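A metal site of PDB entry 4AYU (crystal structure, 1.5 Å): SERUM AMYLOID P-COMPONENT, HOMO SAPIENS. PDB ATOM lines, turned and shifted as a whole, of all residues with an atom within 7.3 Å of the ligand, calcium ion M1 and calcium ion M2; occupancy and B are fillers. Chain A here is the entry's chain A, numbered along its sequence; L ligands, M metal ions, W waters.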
ATOM      1  N   ALA A  46     -40.419   0.345 -25.111  1.00  0.00           N
ATOM      2  CA  ALA A  46     -39.235   0.388 -25.954  1.00  0.00           C
ATOM      3  C   ALA A  46     -38.144  -0.506 -25.393  1.00  0.00           C
ATOM      4  O   ALA A  46     -38.070  -0.760 -24.183  1.00  0.00           O
ATOM      5  CB  ALA A  46     -38.728   1.828 -26.069  1.00  0.00           C
ATOM      6  N   TYR A  47     -37.279  -0.986 -26.264  1.00  0.00           N
ATOM      7  CA  TYR A  47     -36.159  -1.805 -25.847  1.00  0.00           C
ATOM      8  C   TYR A  47     -35.065  -1.866 -26.887  1.00  0.00           C
ATOM      9  O   TYR A  47     -35.320  -1.729 -28.069  1.00  0.00           O
ATOM     10  CB  TYR A  47     -36.626  -3.224 -25.472  1.00  0.00           C
ATOM     11  CG  TYR A  47     -37.423  -3.985 -26.513  1.00  0.00           C
ATOM     12  CD1 TYR A  47     -36.802  -4.729 -27.490  1.00  0.00           C
ATOM     13  CD2 TYR A  47     -38.806  -4.009 -26.453  1.00  0.00           C
ATOM     14  CE1 TYR A  47     -37.540  -5.465 -28.412  1.00  0.00           C
ATOM     15  CE2 TYR A  47     -39.544  -4.737 -27.368  1.00  0.00           C
ATOM     16  CZ  TYR A  47     -38.914  -5.474 -28.336  1.00  0.00           C
ATOM     17  OH  TYR A  47     -39.652  -6.210 -29.258  1.00  0.00           O
ATOM     18  N   SER A  48     -33.844  -2.104 -26.430  1.00  0.00           N
ATOM     19  CA  SER A  48     -32.711  -2.312 -27.292  1.00  0.00           C
ATOM     20  C   SER A  48     -32.633  -3.767 -27.783  1.00  0.00           C
ATOM     21  O   SER A  48     -32.719  -4.718 -26.977  1.00  0.00           O
ATOM     22  CB  SER A  48     -31.412  -1.976 -26.547  1.00  0.00           C
ATOM     23  OG  SER A  48     -30.298  -2.216 -27.374  1.00  0.00           O
ATOM     24  N   SER A  51     -26.895  -3.524 -29.273  1.00  0.00           N
ATOM     25  CA  SER A  51     -26.230  -2.307 -28.797  1.00  0.00           C
ATOM     26  C   SER A  51     -24.721  -2.437 -29.033  1.00  0.00           C
ATOM     27  O   SER A  51     -24.086  -3.326 -28.471  1.00  0.00           O
ATOM     28  CB  SER A  51     -26.531  -2.118 -27.312  1.00  0.00           C
ATOM     29  OG  SER A  51     -25.763  -1.080 -26.712  1.00  0.00           O
ATOM     30  N   ASN A  53     -21.370  -0.043 -28.874  1.00  0.00           N
ATOM     31  CA  ASN A  53     -20.760   1.203 -28.414  1.00  0.00           C
ATOM     32  C   ASN A  53     -19.250   1.091 -28.564  1.00  0.00           C
ATOM     33  O   ASN A  53     -18.676   0.008 -28.505  1.00  0.00           O
ATOM     34  CB  ASN A  53     -21.093   1.453 -26.936  1.00  0.00           C
ATOM     35  CG  ASN A  53     -22.394   2.211 -26.729  1.00  0.00           C
ATOM     36  OD1 ASN A  53     -23.234   2.276 -27.628  1.00  0.00           O
ATOM     37  ND2 ASN A  53     -22.559   2.775 -25.528  1.00  0.00           N
ATOM     38  N   ASP A  58     -21.321   6.723 -27.338  1.00  0.00           N
ATOM     39  CA  ASP A  58     -22.606   6.065 -27.112  1.00  0.00           C
ATOM     40  C   ASP A  58     -23.374   5.959 -28.419  1.00  0.00           C
ATOM     41  O   ASP A  58     -23.183   6.756 -29.324  1.00  0.00           O
ATOM     42  CB  ASP A  58     -23.420   6.852 -26.090  1.00  0.00           C
ATOM     43  CG  ASP A  58     -24.653   6.120 -25.631  1.00  0.00           C
ATOM     44  OD1 ASP A  58     -24.591   4.864 -25.566  1.00  0.00           O
ATOM     45  OD2 ASP A  58     -25.687   6.768 -25.320  1.00  0.00           O
ATOM     46  N   ASN A  59     -24.226   4.942 -28.517  1.00  0.00           N
ATOM     47  CA  ASN A  59     -25.134   4.799 -29.646  1.00  0.00           C
ATOM     48  C   ASN A  59     -24.407   4.838 -30.973  1.00  0.00           C
ATOM     49  O   ASN A  59     -24.850   5.475 -31.931  1.00  0.00           O
ATOM     50  CB  ASN A  59     -26.220   5.870 -29.611  1.00  0.00           C
ATOM     51  CG  ASN A  59     -27.005   5.822 -28.320  1.00  0.00           C
ATOM     52  OD1 ASN A  59     -26.923   4.838 -27.584  1.00  0.00           O
ATOM     53  ND2 ASN A  59     -27.760   6.867 -28.035  1.00  0.00           N
ATOM     54  N   GLU A  60     -23.289   4.140 -31.035  1.00  0.00           N
ATOM     55  CA  GLU A  60     -22.461   4.151 -32.227  1.00  0.00           C
ATOM     56  C   GLU A  60     -23.126   3.326 -33.334  1.00  0.00           C
ATOM     57  O   GLU A  60     -23.105   3.719 -34.505  1.00  0.00           O
ATOM     58  CB  GLU A  60     -21.053   3.661 -31.895  1.00  0.00           C
ATOM     59  CG  GLU A  60     -20.094   3.690 -33.064  1.00  0.00           C
ATOM     60  CD  GLU A  60     -19.766   5.094 -33.555  1.00  0.00           C
ATOM     61  OE1 GLU A  60     -20.125   6.061 -32.875  1.00  0.00           O
ATOM     62  OE2 GLU A  60     -19.163   5.213 -34.624  1.00  0.00           O
ATOM     63  N   LEU A  62     -26.868   1.097 -33.059  1.00  0.00           N
ATOM     64  CA  LEU A  62     -27.894   0.615 -32.147  1.00  0.00           C
ATOM     65  C   LEU A  62     -29.187   0.328 -32.887  1.00  0.00           C
ATOM     66  O   LEU A  62     -29.713   1.172 -33.625  1.00  0.00           O
ATOM     67  CB  LEU A  62     -28.160   1.638 -31.038  1.00  0.00           C
ATOM     68  CG  LEU A  62     -29.421   1.471 -30.190  1.00  0.00           C
ATOM     69  CD1 LEU A  62     -29.332   0.236 -29.294  1.00  0.00           C
ATOM     70  CD2 LEU A  62     -29.664   2.729 -29.328  1.00  0.00           C
ATOM     71  N   TYR A  64     -32.970  -0.416 -32.139  1.00  0.00           N
ATOM     72  CA  TYR A  64     -33.806  -0.071 -31.000  1.00  0.00           C
ATOM     73  C   TYR A  64     -35.267  -0.148 -31.417  1.00  0.00           C
ATOM     74  O   TYR A  64     -35.658   0.429 -32.443  1.00  0.00           O
ATOM     75  CB  TYR A  64     -33.489   1.343 -30.544  1.00  0.00           C
ATOM     76  CG  TYR A  64     -34.093   1.779 -29.224  1.00  0.00           C
ATOM     77  CD1 TYR A  64     -33.589   1.302 -28.026  1.00  0.00           C
ATOM     78  CD2 TYR A  64     -35.105   2.727 -29.172  1.00  0.00           C
ATOM     79  CE1 TYR A  64     -34.098   1.720 -26.823  1.00  0.00           C
ATOM     80  CE2 TYR A  64     -35.636   3.148 -27.958  1.00  0.00           C
ATOM     81  CZ  TYR A  64     -35.121   2.646 -26.793  1.00  0.00           C
ATOM     82  OH  TYR A  64     -35.594   3.061 -25.556  1.00  0.00           O
ATOM     83  N   GLU A  66     -38.905   1.002 -30.835  1.00  0.00           N
ATOM     84  CA  GLU A  66     -39.558   2.122 -30.172  1.00  0.00           C
ATOM     85  C   GLU A  66     -40.900   1.741 -29.534  1.00  0.00           C
ATOM     86  O   GLU A  66     -41.287   2.243 -28.485  1.00  0.00           O
ATOM     87  CB  GLU A  66     -39.838   3.242 -31.190  1.00  0.00           C
ATOM     88  CG  GLU A  66     -38.626   3.741 -31.958  1.00  0.00           C
ATOM     89  CD  GLU A  66     -37.720   4.634 -31.154  1.00  0.00           C
ATOM     90  OE1 GLU A  66     -38.107   5.046 -30.036  1.00  0.00           O
ATOM     91  OE2 GLU A  66     -36.619   4.940 -31.646  1.00  0.00           O
ATOM     92  N   TYR A  74     -29.680   3.599 -34.966  1.00  0.00           N
ATOM     93  CA  TYR A  74     -28.767   4.701 -34.710  1.00  0.00           C
ATOM     94  C   TYR A  74     -27.417   4.367 -35.330  1.00  0.00           C
ATOM     95  O   TYR A  74     -26.941   3.252 -35.187  1.00  0.00           O
ATOM     96  CB  TYR A  74     -28.546   4.934 -33.206  1.00  0.00           C
ATOM     97  CG  TYR A  74     -29.721   5.459 -32.412  1.00  0.00           C
ATOM     98  CD1 TYR A  74     -30.856   4.680 -32.202  1.00  0.00           C
ATOM     99  CD2 TYR A  74     -29.685   6.717 -31.823  1.00  0.00           C
ATOM    100  CE1 TYR A  74     -31.901   5.143 -31.445  1.00  0.00           C
ATOM    101  CE2 TYR A  74     -30.738   7.180 -31.082  1.00  0.00           C
ATOM    102  CZ  TYR A  74     -31.841   6.389 -30.903  1.00  0.00           C
ATOM    103  OH  TYR A  74     -32.896   6.846 -30.154  1.00  0.00           O
ATOM    104  N   LYS A  79     -30.217   9.001 -35.751  1.00  0.00           N
ATOM    105  CA  LYS A  79     -31.168   7.895 -35.883  1.00  0.00           C
ATOM    106  C   LYS A  79     -32.113   8.048 -37.057  1.00  0.00           C
ATOM    107  O   LYS A  79     -32.427   9.170 -37.509  1.00  0.00           O
ATOM    108  CB  LYS A  79     -31.989   7.702 -34.608  1.00  0.00           C
ATOM    109  CG  LYS A  79     -33.019   8.766 -34.387  1.00  0.00           C
ATOM    110  CD  LYS A  79     -33.740   8.641 -33.040  1.00  0.00           C
ATOM    111  CE  LYS A  79     -34.585   7.396 -32.943  1.00  0.00           C
ATOM    112  NZ  LYS A  79     -35.390   7.344 -31.661  1.00  0.00           N
ATOM    113  N   GLU A 136     -29.244  -1.924 -23.237  1.00  0.00           N
ATOM    114  CA  GLU A 136     -28.781  -0.788 -24.016  1.00  0.00           C
ATOM    115  C   GLU A 136     -27.605  -0.149 -23.277  1.00  0.00           C
ATOM    116  O   GLU A 136     -27.747   0.231 -22.127  1.00  0.00           O
ATOM    117  CB  GLU A 136     -29.933   0.212 -24.170  1.00  0.00           C
ATOM    118  CG  GLU A 136     -29.830   1.091 -25.405  1.00  0.00           C
ATOM    119  CD  GLU A 136     -28.847   2.228 -25.263  1.00  0.00           C
ATOM    120  OE1 GLU A 136     -28.826   2.854 -24.180  1.00  0.00           O
ATOM    121  OE2 GLU A 136     -28.098   2.489 -26.223  1.00  0.00           O
ATOM    122  N   GLN A 137     -26.452  -0.065 -23.927  1.00  0.00           N
ATOM    123  CA  GLN A 137     -25.275   0.555 -23.286  1.00  0.00           C
ATOM    124  C   GLN A 137     -25.381   2.061 -23.316  1.00  0.00           C
ATOM    125  O   GLN A 137     -25.789   2.606 -24.321  1.00  0.00           O
ATOM    126  CB  GLN A 137     -23.998   0.183 -24.013  1.00  0.00           C
ATOM    127  CG  GLN A 137     -23.629  -1.267 -24.005  1.00  0.00           C
ATOM    128  CD  GLN A 137     -22.478  -1.567 -24.945  1.00  0.00           C
ATOM    129  OE1 GLN A 137     -21.305  -1.417 -24.589  1.00  0.00           O
ATOM    130  NE2 GLN A 137     -22.810  -1.978 -26.159  1.00  0.00           N
ATOM    131  N   ASP A 138     -24.958   2.718 -22.242  1.00  0.00           N
ATOM    132  CA  ASP A 138     -24.663   4.162 -22.283  1.00  0.00           C
ATOM    133  C   ASP A 138     -23.187   4.464 -22.071  1.00  0.00           C
ATOM    134  O   ASP A 138     -22.771   5.617 -22.164  1.00  0.00           O
ATOM    135  CB  ASP A 138     -25.510   4.917 -21.270  1.00  0.00           C
ATOM    136  CG  ASP A 138     -26.963   4.996 -21.667  1.00  0.00           C
ATOM    137  OD1 ASP A 138     -27.261   4.930 -22.877  1.00  0.00           O
ATOM    138  OD2 ASP A 138     -27.832   5.156 -20.770  1.00  0.00           O
ATOM    139  N   SER A 139     -22.394   3.441 -21.767  1.00  0.00           N
ATOM    140  CA  SER A 139     -20.947   3.570 -21.662  1.00  0.00           C
ATOM    141  C   SER A 139     -20.289   2.478 -22.491  1.00  0.00           C
ATOM    142  O   SER A 139     -20.968   1.724 -23.183  1.00  0.00           O
ATOM    143  CB  SER A 139     -20.524   3.438 -20.203  1.00  0.00           C
ATOM    144  OG  SER A 139     -20.724   2.099 -19.772  1.00  0.00           O
ATOM    145  N   GLY A 142     -21.277  -0.782 -20.508  1.00  0.00           N
ATOM    146  CA  GLY A 142     -22.151  -0.716 -19.355  1.00  0.00           C
ATOM    147  C   GLY A 142     -23.129   0.438 -19.355  1.00  0.00           C
ATOM    148  O   GLY A 142     -23.574   0.885 -20.415  1.00  0.00           O
ATOM    149  N   LYS A 143     -23.472   0.891 -18.148  1.00  0.00           N
ATOM    150  CA  LYS A 143     -24.456   1.944 -17.899  1.00  0.00           C
ATOM    151  C   LYS A 143     -25.765   1.590 -18.579  1.00  0.00           C
ATOM    152  O   LYS A 143     -26.291   2.352 -19.405  1.00  0.00           O
ATOM    153  CB  LYS A 143     -23.926   3.324 -18.321  1.00  0.00           C
ATOM    154  CG  LYS A 143     -22.819   3.844 -17.405  1.00  0.00           C
ATOM    155  CD  LYS A 143     -23.353   4.181 -16.021  1.00  0.00           C
ATOM    156  CE  LYS A 143     -22.264   4.816 -15.157  1.00  0.00           C
ATOM    157  NZ  LYS A 143     -22.707   5.020 -13.746  1.00  0.00           N
ATOM    158  N   PHE A 144     -26.302   0.453 -18.174  1.00  0.00           N
ATOM    159  CA  PHE A 144     -27.555  -0.079 -18.686  1.00  0.00           C
ATOM    160  C   PHE A 144     -28.740   0.620 -18.026  1.00  0.00           C
ATOM    161  O   PHE A 144     -28.590   1.394 -17.078  1.00  0.00           O
ATOM    162  CB  PHE A 144     -27.612  -1.588 -18.427  1.00  0.00           C
ATOM    163  CG  PHE A 144     -26.468  -2.370 -19.008  1.00  0.00           C
ATOM    164  CD1 PHE A 144     -25.940  -2.057 -20.248  1.00  0.00           C
ATOM    165  CD2 PHE A 144     -25.915  -3.427 -18.303  1.00  0.00           C
ATOM    166  CE1 PHE A 144     -24.908  -2.786 -20.783  1.00  0.00           C
ATOM    167  CE2 PHE A 144     -24.874  -4.172 -18.835  1.00  0.00           C
ATOM    168  CZ  PHE A 144     -24.374  -3.848 -20.086  1.00  0.00           C
ATOM    169  N   ASP A 145     -29.940   0.331 -18.540  1.00  0.00           N
ATOM    170  CA  ASP A 145     -31.174   0.977 -18.103  1.00  0.00           C
ATOM    171  C   ASP A 145     -32.287  -0.069 -18.181  1.00  0.00           C
ATOM    172  O   ASP A 145     -32.642  -0.535 -19.272  1.00  0.00           O
ATOM    173  CB  ASP A 145     -31.459   2.173 -19.013  1.00  0.00           C
ATOM    174  CG  ASP A 145     -32.770   2.895 -18.691  1.00  0.00           C
ATOM    175  OD1 ASP A 145     -33.600   2.387 -17.904  1.00  0.00           O
ATOM    176  OD2 ASP A 145     -32.982   3.969 -19.270  1.00  0.00           O
ATOM    177  N   GLN A 148     -35.005  -0.078 -20.811  1.00  0.00           N
ATOM    178  CA  GLN A 148     -34.609  -0.367 -22.186  1.00  0.00           C
ATOM    179  C   GLN A 148     -34.144  -1.810 -22.352  1.00  0.00           C
ATOM    180  O   GLN A 148     -33.696  -2.193 -23.444  1.00  0.00           O
ATOM    181  CB  GLN A 148     -33.504   0.577 -22.624  1.00  0.00           C
ATOM    182  CG  GLN A 148     -33.900   2.040 -22.572  1.00  0.00           C
ATOM    183  CD  GLN A 148     -32.769   2.989 -22.972  1.00  0.00           C
ATOM    184  OE1 GLN A 148     -31.646   2.865 -22.505  1.00  0.00           O
ATOM    185  NE2 GLN A 148     -33.081   3.935 -23.840  1.00  0.00           N
HETATM  186  C1  LIG L   1     -32.884   7.550 -25.101  1.00  0.00           C
HETATM  187  O1  LIG L   1     -34.104   7.604 -24.889  1.00  0.00           O
HETATM  188  C2  LIG L   1     -31.937   8.474 -24.422  1.00  0.00           C
HETATM  189  N1  LIG L   1     -32.364   6.580 -26.004  1.00  0.00           N
HETATM  190  C3  LIG L   1     -30.976   6.433 -26.339  1.00  0.00           C
HETATM  191  C4  LIG L   1     -30.947   5.489 -27.503  1.00  0.00           C
HETATM  192  C5  LIG L   1     -32.176   4.683 -27.381  1.00  0.00           C
HETATM  193  C6  LIG L   1     -33.174   5.627 -26.742  1.00  0.00           C
HETATM  194  C7  LIG L   1     -30.111   5.917 -25.222  1.00  0.00           C
HETATM  195  O2  LIG L   1     -30.646   5.423 -24.186  1.00  0.00           O
HETATM  196  O3  LIG L   1     -28.858   5.977 -25.337  1.00  0.00           O
HETATM  197 CA    CA M   1     -27.031   4.448 -25.203  1.00  0.00          CA
HETATM  198 CA    CA M   2     -29.632   4.225 -22.402  1.00  0.00          CA
HETATM  199  O   HOH W   1     -28.749   2.450 -20.961  1.00  0.00           O
HETATM  200  O   HOH W   2     -31.074   5.164 -20.703  1.00  0.00           O
HETATM  201  O   HOH W   3     -27.608   8.199 -23.040  1.00  0.00           O
HETATM  202  O   HOH W   4     -29.820   6.945 -22.225  1.00  0.00           O
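O of Lys 143 sits at hydrogen-bond distance from N of Asp 138, at 3.2 Å.
The backbone carbonyl oxygen (O) of Gln 137 sits close to the side-chain amide nitrogen (ND2) of Asn 53 (3.5 Å).
The side-chain amide nitrogen (NE2) of Gln 137 lies within hydrogen-bond range of the backbone carbonyl oxygen (O) of Ser 51.
OD1 of Asn 53 lies within hydrogen-bond range of N of Asn 59, at 3.0 Å.
The side-chain amide nitrogen of Gln 148 sits at hydrogen-bond distance from the side-chain hydroxyl of Tyr 64 (3.2 Å).
The backbone carbonyl oxygen (O) of Gln 148 lies within hydrogen-bond range of the backbone NH (N) of Ser 48 (3.0 Å).
OD1 of Asp 58 lies close to ND2 of Asn 53.
NZ of Lys 79 is in hydrogen-bond range of OH of Tyr 74 (3.0 Å).
Leu 62 touches the ligand (CD2 to C4, 3.5 Å).
CZ of Tyr 64 touches C6 of the ligand, at 3.6 Å.
OH of Tyr 74 touches C4 of the ligand, 3.6 Å away.
The nearest printed residue that does not touch the ligand is Gln 137 (4.7 Å).
Five residues have an atom within 4 Å of calcium ion M1: Asp 58, Asn 59, Glu 136, Gln 137 and Asp 138.
Along chain A the residues within 4 Å of calcium ion M1 span positions 58 to 138.
Of the 22 residues printed, 3 come within 4 Å of calcium ion M2.
The nearest printed residue that does not touch calcium ion M2 is Asp 145 (4.4 Å).
Calcium ion M1 is bound by the side-chain carboxylate (OD1) of Asp 138 (2.4 Å), an oxygen (O3) of the ligand (2.4 Å), the backbone carbonyl oxygen (O) of Gln 137 (2.4 Å), the side-chain amide oxygen (OD1) of Asn 59 (2.4 Å), the side-chain carboxylate (OE2) of Glu 136 (2.5 Å), the side-chain carboxylate (OD1) of Asp 58 (2.5 Å), the side-chain carboxylate (OE1) of Glu 136 (2.6 Å) and the side-chain carboxylate (OD2) of Asp 58 (2.7 Å).
An oxygen (O2) of the ligand is bound to calcium ion M2, 2.4 Å away.
The side-chain carboxylate (OE1) of Glu 136 is bound to calcium ion M2 (2.4 Å).
Calcium ion M2 is bound by water W2, at 2.4 Å.
OE1 of Gln 148 is bound to calcium ion M2, at 2.4 Å.
Water W1 binds calcium ion M2 (2.5 Å).
OD1 of Asp 138 is bound to calcium ion M2, at 2.5 Å.
Calcium ion M2 is bound by OD2 of Asp 138, 2.6 Å away.
Water W4 is bound to calcium ion M2, at 2.7 Å.
Calcium ion M2 has eight donor atoms within binding distance.
Water W1 lies within hydrogen-bond range of the backbone carbonyl oxygen of Glu 136 (2.7 Å), the backbone carbonyl oxygen of Lys 143 (2.9 Å) and the backbone NH of Asp 145 (3.4 Å).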
